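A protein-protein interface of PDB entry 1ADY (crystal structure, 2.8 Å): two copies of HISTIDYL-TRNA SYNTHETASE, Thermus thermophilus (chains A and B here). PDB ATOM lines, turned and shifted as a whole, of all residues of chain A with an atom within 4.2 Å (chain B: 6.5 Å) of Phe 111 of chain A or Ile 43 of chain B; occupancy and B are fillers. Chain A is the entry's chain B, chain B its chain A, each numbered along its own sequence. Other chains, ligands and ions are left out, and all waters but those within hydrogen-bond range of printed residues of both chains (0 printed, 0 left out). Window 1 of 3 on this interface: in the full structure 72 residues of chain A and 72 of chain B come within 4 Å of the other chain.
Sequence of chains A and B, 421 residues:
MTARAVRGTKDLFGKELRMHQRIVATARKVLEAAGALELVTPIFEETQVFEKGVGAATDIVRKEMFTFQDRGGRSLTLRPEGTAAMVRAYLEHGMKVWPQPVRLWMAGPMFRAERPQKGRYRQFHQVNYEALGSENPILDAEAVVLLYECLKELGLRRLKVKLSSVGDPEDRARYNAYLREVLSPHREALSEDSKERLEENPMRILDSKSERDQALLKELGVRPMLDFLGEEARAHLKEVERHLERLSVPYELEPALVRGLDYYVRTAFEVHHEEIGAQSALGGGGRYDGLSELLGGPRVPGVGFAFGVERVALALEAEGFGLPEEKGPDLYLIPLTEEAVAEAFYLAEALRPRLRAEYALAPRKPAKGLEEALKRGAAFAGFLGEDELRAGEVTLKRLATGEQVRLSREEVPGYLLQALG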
ATOM      1  N   ILE A  43     -29.156 -12.184 -20.773  1.00  0.00           N
ATOM      2  CA  ILE A  43     -28.002 -12.118 -19.882  1.00  0.00           C
ATOM      3  C   ILE A  43     -26.720 -11.743 -20.637  1.00  0.00           C
ATOM      4  O   ILE A  43     -25.775 -11.206 -20.051  1.00  0.00           O
ATOM      5  CB  ILE A  43     -27.819 -13.468 -19.131  1.00  0.00           C
ATOM      6  CG1 ILE A  43     -28.987 -13.686 -18.164  1.00  0.00           C
ATOM      7  CG2 ILE A  43     -26.479 -13.519 -18.392  1.00  0.00           C
ATOM      8  CD1 ILE A  43     -29.008 -12.742 -16.973  1.00  0.00           C
ATOM      9  N   PHE A  66     -16.955 -10.211 -18.688  1.00  0.00           N
ATOM     10  CA  PHE A  66     -16.927 -11.664 -18.793  1.00  0.00           C
ATOM     11  C   PHE A  66     -17.352 -11.972 -20.221  1.00  0.00           C
ATOM     12  O   PHE A  66     -18.541 -12.043 -20.529  1.00  0.00           O
ATOM     13  CB  PHE A  66     -17.893 -12.306 -17.795  1.00  0.00           C
ATOM     14  CG  PHE A  66     -17.404 -12.280 -16.376  1.00  0.00           C
ATOM     15  CD1 PHE A  66     -16.181 -12.852 -16.037  1.00  0.00           C
ATOM     16  CD2 PHE A  66     -18.165 -11.691 -15.378  1.00  0.00           C
ATOM     17  CE1 PHE A  66     -15.729 -12.837 -14.721  1.00  0.00           C
ATOM     18  CE2 PHE A  66     -17.720 -11.669 -14.061  1.00  0.00           C
ATOM     19  CZ  PHE A  66     -16.502 -12.243 -13.732  1.00  0.00           C
ATOM     20  N   LEU A  78     -21.143 -11.272 -21.027  1.00  0.00           N
ATOM     21  CA  LEU A  78     -22.080 -11.228 -19.919  1.00  0.00           C
ATOM     22  C   LEU A  78     -22.360  -9.766 -19.608  1.00  0.00           C
ATOM     23  O   LEU A  78     -21.447  -9.016 -19.251  1.00  0.00           O
ATOM     24  CB  LEU A  78     -21.467 -11.908 -18.693  1.00  0.00           C
ATOM     25  CG  LEU A  78     -22.012 -13.279 -18.291  1.00  0.00           C
ATOM     26  CD1 LEU A  78     -22.143 -14.194 -19.496  1.00  0.00           C
ATOM     27  CD2 LEU A  78     -21.098 -13.879 -17.238  1.00  0.00           C
ATOM     28  N   ARG A  79     -23.616  -9.369 -19.776  1.00  0.00           N
ATOM     29  CA  ARG A  79     -24.067  -7.999 -19.526  1.00  0.00           C
ATOM     30  C   ARG A  79     -23.515  -7.368 -18.244  1.00  0.00           C
ATOM     31  O   ARG A  79     -23.777  -7.841 -17.138  1.00  0.00           O
ATOM     32  CB  ARG A  79     -25.600  -7.964 -19.545  1.00  0.00           C
ATOM     33  CG  ARG A  79     -26.237  -7.001 -18.572  1.00  0.00           C
ATOM     34  CD  ARG A  79     -27.214  -7.733 -17.654  1.00  0.00           C
ATOM     35  NE  ARG A  79     -28.477  -8.043 -18.319  1.00  0.00           N
ATOM     36  CZ  ARG A  79     -29.585  -8.419 -17.684  1.00  0.00           C
ATOM     37  NH1 ARG A  79     -29.593  -8.540 -16.362  1.00  0.00           N
ATOM     38  NH2 ARG A  79     -30.703  -8.631 -18.367  1.00  0.00           N
ATOM     39  N   PRO A  80     -22.690  -6.315 -18.393  1.00  0.00           N
ATOM     40  CA  PRO A  80     -22.091  -5.599 -17.256  1.00  0.00           C
ATOM     41  C   PRO A  80     -22.910  -4.378 -16.844  1.00  0.00           C
ATOM     42  O   PRO A  80     -22.752  -3.858 -15.735  1.00  0.00           O
ATOM     43  CB  PRO A  80     -20.741  -5.175 -17.823  1.00  0.00           C
ATOM     44  CG  PRO A  80     -21.088  -4.819 -19.223  1.00  0.00           C
ATOM     45  CD  PRO A  80     -22.037  -5.931 -19.654  1.00  0.00           C
ATOM     46  N   PRO A 109     -29.557  -9.341 -12.790  1.00  0.00           N
ATOM     47  CA  PRO A 109     -28.142  -9.451 -12.444  1.00  0.00           C
ATOM     48  C   PRO A 109     -27.228  -8.832 -13.500  1.00  0.00           C
ATOM     49  O   PRO A 109     -27.545  -8.832 -14.689  1.00  0.00           O
ATOM     50  CB  PRO A 109     -27.947 -10.962 -12.342  1.00  0.00           C
ATOM     51  CG  PRO A 109     -28.844 -11.466 -13.428  1.00  0.00           C
ATOM     52  CD  PRO A 109     -30.097 -10.640 -13.231  1.00  0.00           C
ATOM     53  N   MET A 110     -26.110  -8.284 -13.040  1.00  0.00           N
ATOM     54  CA  MET A 110     -25.113  -7.676 -13.909  1.00  0.00           C
ATOM     55  C   MET A 110     -23.804  -8.335 -13.507  1.00  0.00           C
ATOM     56  O   MET A 110     -23.604  -8.655 -12.330  1.00  0.00           O
ATOM     57  CB  MET A 110     -25.033  -6.170 -13.667  1.00  0.00           C
ATOM     58  CG  MET A 110     -26.288  -5.394 -14.002  1.00  0.00           C
ATOM     59  SD  MET A 110     -26.649  -5.373 -15.764  1.00  0.00           S
ATOM     60  CE  MET A 110     -28.360  -4.839 -15.765  1.00  0.00           C
ATOM     61  N   PHE A 111     -22.906  -8.511 -14.467  1.00  0.00           N
ATOM     62  CA  PHE A 111     -21.637  -9.168 -14.199  1.00  0.00           C
ATOM     63  C   PHE A 111     -20.436  -8.325 -14.597  1.00  0.00           C
ATOM     64  O   PHE A 111     -20.293  -7.933 -15.760  1.00  0.00           O
ATOM     65  CB  PHE A 111     -21.602 -10.516 -14.926  1.00  0.00           C
ATOM     66  CG  PHE A 111     -22.941 -11.194 -14.994  1.00  0.00           C
ATOM     67  CD1 PHE A 111     -23.368 -12.027 -13.966  1.00  0.00           C
ATOM     68  CD2 PHE A 111     -23.804 -10.943 -16.055  1.00  0.00           C
ATOM     69  CE1 PHE A 111     -24.632 -12.593 -13.991  1.00  0.00           C
ATOM     70  CE2 PHE A 111     -25.068 -11.506 -16.087  1.00  0.00           C
ATOM     71  CZ  PHE A 111     -25.485 -12.333 -15.050  1.00  0.00           C
ATOM     72  N   ARG A 112     -19.571  -8.067 -13.623  1.00  0.00           N
ATOM     73  CA  ARG A 112     -18.366  -7.283 -13.845  1.00  0.00           C
ATOM     74  C   ARG A 112     -17.162  -8.056 -13.328  1.00  0.00           C
ATOM     75  O   ARG A 112     -17.092  -8.387 -12.147  1.00  0.00           O
ATOM     76  CB  ARG A 112     -18.462  -5.934 -13.132  1.00  0.00           C
ATOM     77  CG  ARG A 112     -18.367  -4.751 -14.078  1.00  0.00           C
ATOM     78  CD  ARG A 112     -19.719  -4.104 -14.309  1.00  0.00           C
ATOM     79  NE  ARG A 112     -19.967  -3.049 -13.334  1.00  0.00           N
ATOM     80  CZ  ARG A 112     -20.674  -1.948 -13.582  1.00  0.00           C
ATOM     81  NH1 ARG A 112     -21.220  -1.748 -14.774  1.00  0.00           N
ATOM     82  NH2 ARG A 112     -20.792  -1.017 -12.647  1.00  0.00           N
ATOM     83  N   ARG A 122     -18.951  -9.592  -8.113  1.00  0.00           N
ATOM     84  CA  ARG A 122     -18.731  -9.917  -9.518  1.00  0.00           C
ATOM     85  C   ARG A 122     -20.089 -10.089 -10.187  1.00  0.00           C
ATOM     86  O   ARG A 122     -20.234  -9.900 -11.399  1.00  0.00           O
ATOM     87  CB  ARG A 122     -17.855 -11.160  -9.675  1.00  0.00           C
ATOM     88  CG  ARG A 122     -16.447 -10.805 -10.129  1.00  0.00           C
ATOM     89  CD  ARG A 122     -15.391 -11.369  -9.207  1.00  0.00           C
ATOM     90  NE  ARG A 122     -15.174 -12.789  -9.433  1.00  0.00           N
ATOM     91  CZ  ARG A 122     -14.512 -13.287 -10.475  1.00  0.00           C
ATOM     92  NH1 ARG A 122     -13.993 -12.485 -11.403  1.00  0.00           N
ATOM     93  NH2 ARG A 122     -14.369 -14.597 -10.592  1.00  0.00           N
ATOM     94  N   GLN A 123     -21.073 -10.473  -9.380  1.00  0.00           N
ATOM     95  CA  GLN A 123     -22.443 -10.611  -9.844  1.00  0.00           C
ATOM     96  C   GLN A 123     -23.292  -9.835  -8.854  1.00  0.00           C
ATOM     97  O   GLN A 123     -23.366 -10.182  -7.670  1.00  0.00           O
ATOM     98  CB  GLN A 123     -22.927 -12.062  -9.892  1.00  0.00           C
ATOM     99  CG  GLN A 123     -24.352 -12.140 -10.451  1.00  0.00           C
ATOM    100  CD  GLN A 123     -25.014 -13.491 -10.302  1.00  0.00           C
ATOM    101  OE1 GLN A 123     -24.518 -14.502 -10.793  1.00  0.00           O
ATOM    102  NE2 GLN A 123     -26.166 -13.509  -9.651  1.00  0.00           N
ATOM    103  N   THR B  41     -29.314 -19.447  -6.819  1.00  0.00           N
ATOM    104  CA  THR B  41     -27.887 -19.629  -7.007  1.00  0.00           C
ATOM    105  C   THR B  41     -27.374 -18.701  -8.106  1.00  0.00           C
ATOM    106  O   THR B  41     -28.161 -18.169  -8.900  1.00  0.00           O
ATOM    107  CB  THR B  41     -27.553 -21.087  -7.372  1.00  0.00           C
ATOM    108  OG1 THR B  41     -28.336 -21.491  -8.502  1.00  0.00           O
ATOM    109  CG2 THR B  41     -27.841 -22.005  -6.202  1.00  0.00           C
ATOM    110  N   PRO B  42     -26.052 -18.452  -8.125  1.00  0.00           N
ATOM    111  CA  PRO B  42     -25.406 -17.589  -9.115  1.00  0.00           C
ATOM    112  C   PRO B  42     -25.609 -18.094 -10.539  1.00  0.00           C
ATOM    113  O   PRO B  42     -25.820 -19.285 -10.758  1.00  0.00           O
ATOM    114  CB  PRO B  42     -23.939 -17.662  -8.712  1.00  0.00           C
ATOM    115  CG  PRO B  42     -24.017 -17.813  -7.232  1.00  0.00           C
ATOM    116  CD  PRO B  42     -25.083 -18.857  -7.092  1.00  0.00           C
ATOM    117  N   ILE B  43     -25.523 -17.179 -11.501  1.00  0.00           N
ATOM    118  CA  ILE B  43     -25.682 -17.498 -12.915  1.00  0.00           C
ATOM    119  C   ILE B  43     -24.600 -18.466 -13.409  1.00  0.00           C
ATOM    120  O   ILE B  43     -24.804 -19.193 -14.386  1.00  0.00           O
ATOM    121  CB  ILE B  43     -25.677 -16.200 -13.763  1.00  0.00           C
ATOM    122  CG1 ILE B  43     -26.929 -15.378 -13.452  1.00  0.00           C
ATOM    123  CG2 ILE B  43     -25.591 -16.510 -15.256  1.00  0.00           C
ATOM    124  CD1 ILE B  43     -28.226 -16.000 -13.934  1.00  0.00           C
ATOM    125  N   PHE B  44     -23.446 -18.462 -12.750  1.00  0.00           N
ATOM    126  CA  PHE B  44     -22.364 -19.361 -13.124  1.00  0.00           C
ATOM    127  C   PHE B  44     -21.710 -20.020 -11.914  1.00  0.00           C
ATOM    128  O   PHE B  44     -21.742 -19.490 -10.793  1.00  0.00           O
ATOM    129  CB  PHE B  44     -21.318 -18.652 -14.007  1.00  0.00           C
ATOM    130  CG  PHE B  44     -20.851 -17.318 -13.474  1.00  0.00           C
ATOM    131  CD1 PHE B  44     -20.134 -17.229 -12.283  1.00  0.00           C
ATOM    132  CD2 PHE B  44     -21.112 -16.150 -14.182  1.00  0.00           C
ATOM    133  CE1 PHE B  44     -19.683 -16.001 -11.805  1.00  0.00           C
ATOM    134  CE2 PHE B  44     -20.665 -14.912 -13.713  1.00  0.00           C
ATOM    135  CZ  PHE B  44     -19.949 -14.841 -12.521  1.00  0.00           C
ATOM    136  N   GLU B  45     -21.157 -21.203 -12.143  1.00  0.00           N
ATOM    137  CA  GLU B  45     -20.487 -21.963 -11.096  1.00  0.00           C
ATOM    138  C   GLU B  45     -19.143 -22.408 -11.660  1.00  0.00           C
ATOM    139  O   GLU B  45     -18.876 -22.215 -12.851  1.00  0.00           O
ATOM    140  CB  GLU B  45     -21.310 -23.210 -10.731  1.00  0.00           C
ATOM    141  CG  GLU B  45     -22.739 -22.949 -10.240  1.00  0.00           C
ATOM    142  CD  GLU B  45     -22.864 -22.803  -8.724  1.00  0.00           C
ATOM    143  OE1 GLU B  45     -21.835 -22.835  -8.008  1.00  0.00           O
ATOM    144  OE2 GLU B  45     -24.014 -22.668  -8.249  1.00  0.00           O
ATOM    145  N   PHE B  50     -20.624 -28.660 -12.888  1.00  0.00           N
ATOM    146  CA  PHE B  50     -21.462 -29.196 -13.952  1.00  0.00           C
ATOM    147  C   PHE B  50     -20.844 -30.412 -14.643  1.00  0.00           C
ATOM    148  O   PHE B  50     -21.566 -31.325 -15.039  1.00  0.00           O
ATOM    149  CB  PHE B  50     -21.812 -28.100 -14.959  1.00  0.00           C
ATOM    150  CG  PHE B  50     -22.574 -26.955 -14.356  1.00  0.00           C
ATOM    151  CD1 PHE B  50     -23.823 -27.161 -13.772  1.00  0.00           C
ATOM    152  CD2 PHE B  50     -22.034 -25.671 -14.339  1.00  0.00           C
ATOM    153  CE1 PHE B  50     -24.523 -26.108 -13.179  1.00  0.00           C
ATOM    154  CE2 PHE B  50     -22.725 -24.607 -13.747  1.00  0.00           C
ATOM    155  CZ  PHE B  50     -23.971 -24.827 -13.167  1.00  0.00           C
ATOM    156  N   THR B  77     -18.675 -21.682 -15.735  1.00  0.00           N
ATOM    157  CA  THR B  77     -19.653 -22.055 -16.746  1.00  0.00           C
ATOM    158  C   THR B  77     -21.044 -21.514 -16.428  1.00  0.00           C
ATOM    159  O   THR B  77     -21.477 -21.476 -15.268  1.00  0.00           O
ATOM    160  CB  THR B  77     -19.722 -23.582 -16.928  1.00  0.00           C
ATOM    161  OG1 THR B  77     -18.426 -24.077 -17.281  1.00  0.00           O
ATOM    162  CG2 THR B  77     -20.692 -23.945 -18.032  1.00  0.00           C
ATOM    163  N   LEU B  78     -21.709 -21.036 -17.473  1.00  0.00           N
ATOM    164  CA  LEU B  78     -23.056 -20.505 -17.376  1.00  0.00           C
ATOM    165  C   LEU B  78     -23.985 -21.660 -17.060  1.00  0.00           C
ATOM    166  O   LEU B  78     -24.091 -22.608 -17.837  1.00  0.00           O
ATOM    167  CB  LEU B  78     -23.463 -19.866 -18.704  1.00  0.00           C
ATOM    168  CG  LEU B  78     -23.529 -18.336 -18.786  1.00  0.00           C
ATOM    169  CD1 LEU B  78     -22.294 -17.713 -18.163  1.00  0.00           C
ATOM    170  CD2 LEU B  78     -23.690 -17.903 -20.235  1.00  0.00           C
ATOM    171  N   ARG B  79     -24.617 -21.589 -15.896  1.00  0.00           N
ATOM    172  CA  ARG B  79     -25.546 -22.611 -15.426  1.00  0.00           C
ATOM    173  C   ARG B  79     -26.517 -23.134 -16.491  1.00  0.00           C
ATOM    174  O   ARG B  79     -27.337 -22.382 -17.028  1.00  0.00           O
ATOM    175  CB  ARG B  79     -26.304 -22.074 -14.204  1.00  0.00           C
ATOM    176  CG  ARG B  79     -27.737 -22.531 -14.068  1.00  0.00           C
ATOM    177  CD  ARG B  79     -28.671 -21.334 -13.981  1.00  0.00           C
ATOM    178  NE  ARG B  79     -28.662 -20.718 -12.658  1.00  0.00           N
ATOM    179  CZ  ARG B  79     -29.557 -19.827 -12.244  1.00  0.00           C
ATOM    180  NH1 ARG B  79     -30.540 -19.442 -13.049  1.00  0.00           N
ATOM    181  NH2 ARG B  79     -29.482 -19.337 -11.014  1.00  0.00           N
ATOM    182  N   PRO B  80     -26.392 -24.424 -16.849  1.00  0.00           N
ATOM    183  CA  PRO B  80     -27.251 -25.070 -17.849  1.00  0.00           C
ATOM    184  C   PRO B  80     -28.439 -25.793 -17.206  1.00  0.00           C
ATOM    185  O   PRO B  80     -29.424 -26.105 -17.882  1.00  0.00           O
ATOM    186  CB  PRO B  80     -26.300 -26.065 -18.502  1.00  0.00           C
ATOM    187  CG  PRO B  80     -25.491 -26.535 -17.350  1.00  0.00           C
ATOM    188  CD  PRO B  80     -25.211 -25.261 -16.558  1.00  0.00           C
ATOM    189  N   GLY B 108     -35.432 -19.120 -12.716  1.00  0.00           N
ATOM    190  CA  GLY B 108     -34.420 -18.269 -13.314  1.00  0.00           C
ATOM    191  C   GLY B 108     -34.006 -18.725 -14.693  1.00  0.00           C
ATOM    192  O   GLY B 108     -34.598 -19.654 -15.252  1.00  0.00           O
ATOM    193  N   PRO B 109     -33.048 -18.026 -15.309  1.00  0.00           N
ATOM    194  CA  PRO B 109     -32.579 -18.389 -16.645  1.00  0.00           C
ATOM    195  C   PRO B 109     -31.534 -19.504 -16.626  1.00  0.00           C
ATOM    196  O   PRO B 109     -30.752 -19.627 -15.678  1.00  0.00           O
ATOM    197  CB  PRO B 109     -31.992 -17.076 -17.154  1.00  0.00           C
ATOM    198  CG  PRO B 109     -31.401 -16.481 -15.907  1.00  0.00           C
ATOM    199  CD  PRO B 109     -32.496 -16.725 -14.887  1.00  0.00           C
ATOM    200  N   PHE B 111     -28.764 -21.594 -19.400  1.00  0.00           N
ATOM    201  CA  PHE B 111     -28.098 -21.414 -20.681  1.00  0.00           C
ATOM    202  C   PHE B 111     -27.499 -22.698 -21.226  1.00  0.00           C
ATOM    203  O   PHE B 111     -26.647 -23.332 -20.591  1.00  0.00           O
ATOM    204  CB  PHE B 111     -27.008 -20.352 -20.534  1.00  0.00           C
ATOM    205  CG  PHE B 111     -27.371 -19.257 -19.568  1.00  0.00           C
ATOM    206  CD1 PHE B 111     -28.094 -18.145 -19.998  1.00  0.00           C
ATOM    207  CD2 PHE B 111     -27.047 -19.375 -18.217  1.00  0.00           C
ATOM    208  CE1 PHE B 111     -28.492 -17.170 -19.098  1.00  0.00           C
ATOM    209  CE2 PHE B 111     -27.441 -18.403 -17.307  1.00  0.00           C
ATOM    210  CZ  PHE B 111     -28.167 -17.298 -17.745  1.00  0.00           C
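Printed residues of chain B that touch a printed residue of chain A: Pro 42, Ile 43, Phe 44, Leu 78 and Phe 111.
Hydrophobic or aromatic side chains of chain B that line the printed part of chain A: Pro 42, Ile 43, Phe 44, Leu 78 and Phe 111.
Along chain B the printed residues that touch a printed residue of chain A span positions 42 to 111.
Among the printed residues, no Asp or Glu carboxylate lies within 4 Å of a Lys or Arg side-chain nitrogen of the other chain.
The backbone carbonyl oxygen of Ile 43 of chain B is in hydrogen-bond range of the backbone NH of Arg 79 of chain B (2.8 Å).
N of Phe 111 of chain B is in hydrogen-bond range of O of Arg 79 of chain B, at 2.9 Å.
The backbone carbonyl oxygen (O) of Ile 43 of chain A sits at hydrogen-bond distance from the backbone NH (N) of Arg 79 of chain A.
O of Phe 66 of chain A lies within hydrogen-bond range of N of Leu 78 of chain A (2.8 Å).
The backbone NH of Phe 111 of chain A sits at hydrogen-bond distance from the backbone carbonyl oxygen of Arg 79 of chain A, 2.9 Å away.
Ile 43 of chain A touches Phe 111 of chain B, and with the chains exchanged Phe 111 of chain A touches Ile 43 of chain B.
Leu 78 of chain B touches its own counterpart, Leu 78 of chain A.
6 positions are printed for both chains.
Of the 7 pairs that touch across the chains among the printed residues, 3 have their exchanged pair printed and touching as well.
Ile 43 of chain B touches just these residues of chain A: Phe 111 (3.7 Å) and Gln 123 (2.9 Å).
Printed residues of chain A within 4 Å of Phe 44 of chain B: Leu 78 (3.7 Å) and Phe 111 (3.96 Å).
Printed residues of chain A within 4 Å of Leu 78 of chain B: Leu 78.
Of the printed residues of chain B, Gln 123 of chain A touches Pro 42 (3.6 Å) and Ile 43 (2.9 Å).
The nearest residue of chain B that does not touch Phe 111 of chain A is Phe 111 of chain B (6.3 Å).
The nearest printed residue of chain A that does not touch Ile 43 of chain B is Pro 109 of chain A (4.4 Å).
The side-chain amide oxygen of Gln 123 of chain A sits at hydrogen-bond distance from the backbone NH of Ile 43 of chain B (2.9 Å).
CE1 of Phe 111 of chain B touches CG1 of Ile 43 of chain A, at 3.6 Å.
Phe 44 of chain B touches Leu 78 of chain A (CE2 to CD2, 3.7 Å).
Leu 78 of chain B touches Leu 78 of chain A.
Phe 111 of chain A touches Ile 43 of chain B.
CD1 of Phe 111 of chain A touches CE2 of Phe 44 of chain B, 3.96 Å away.
Gln 123 of chain A touches Pro 42 of chain B (OE1 to CA, 3.6 Å).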
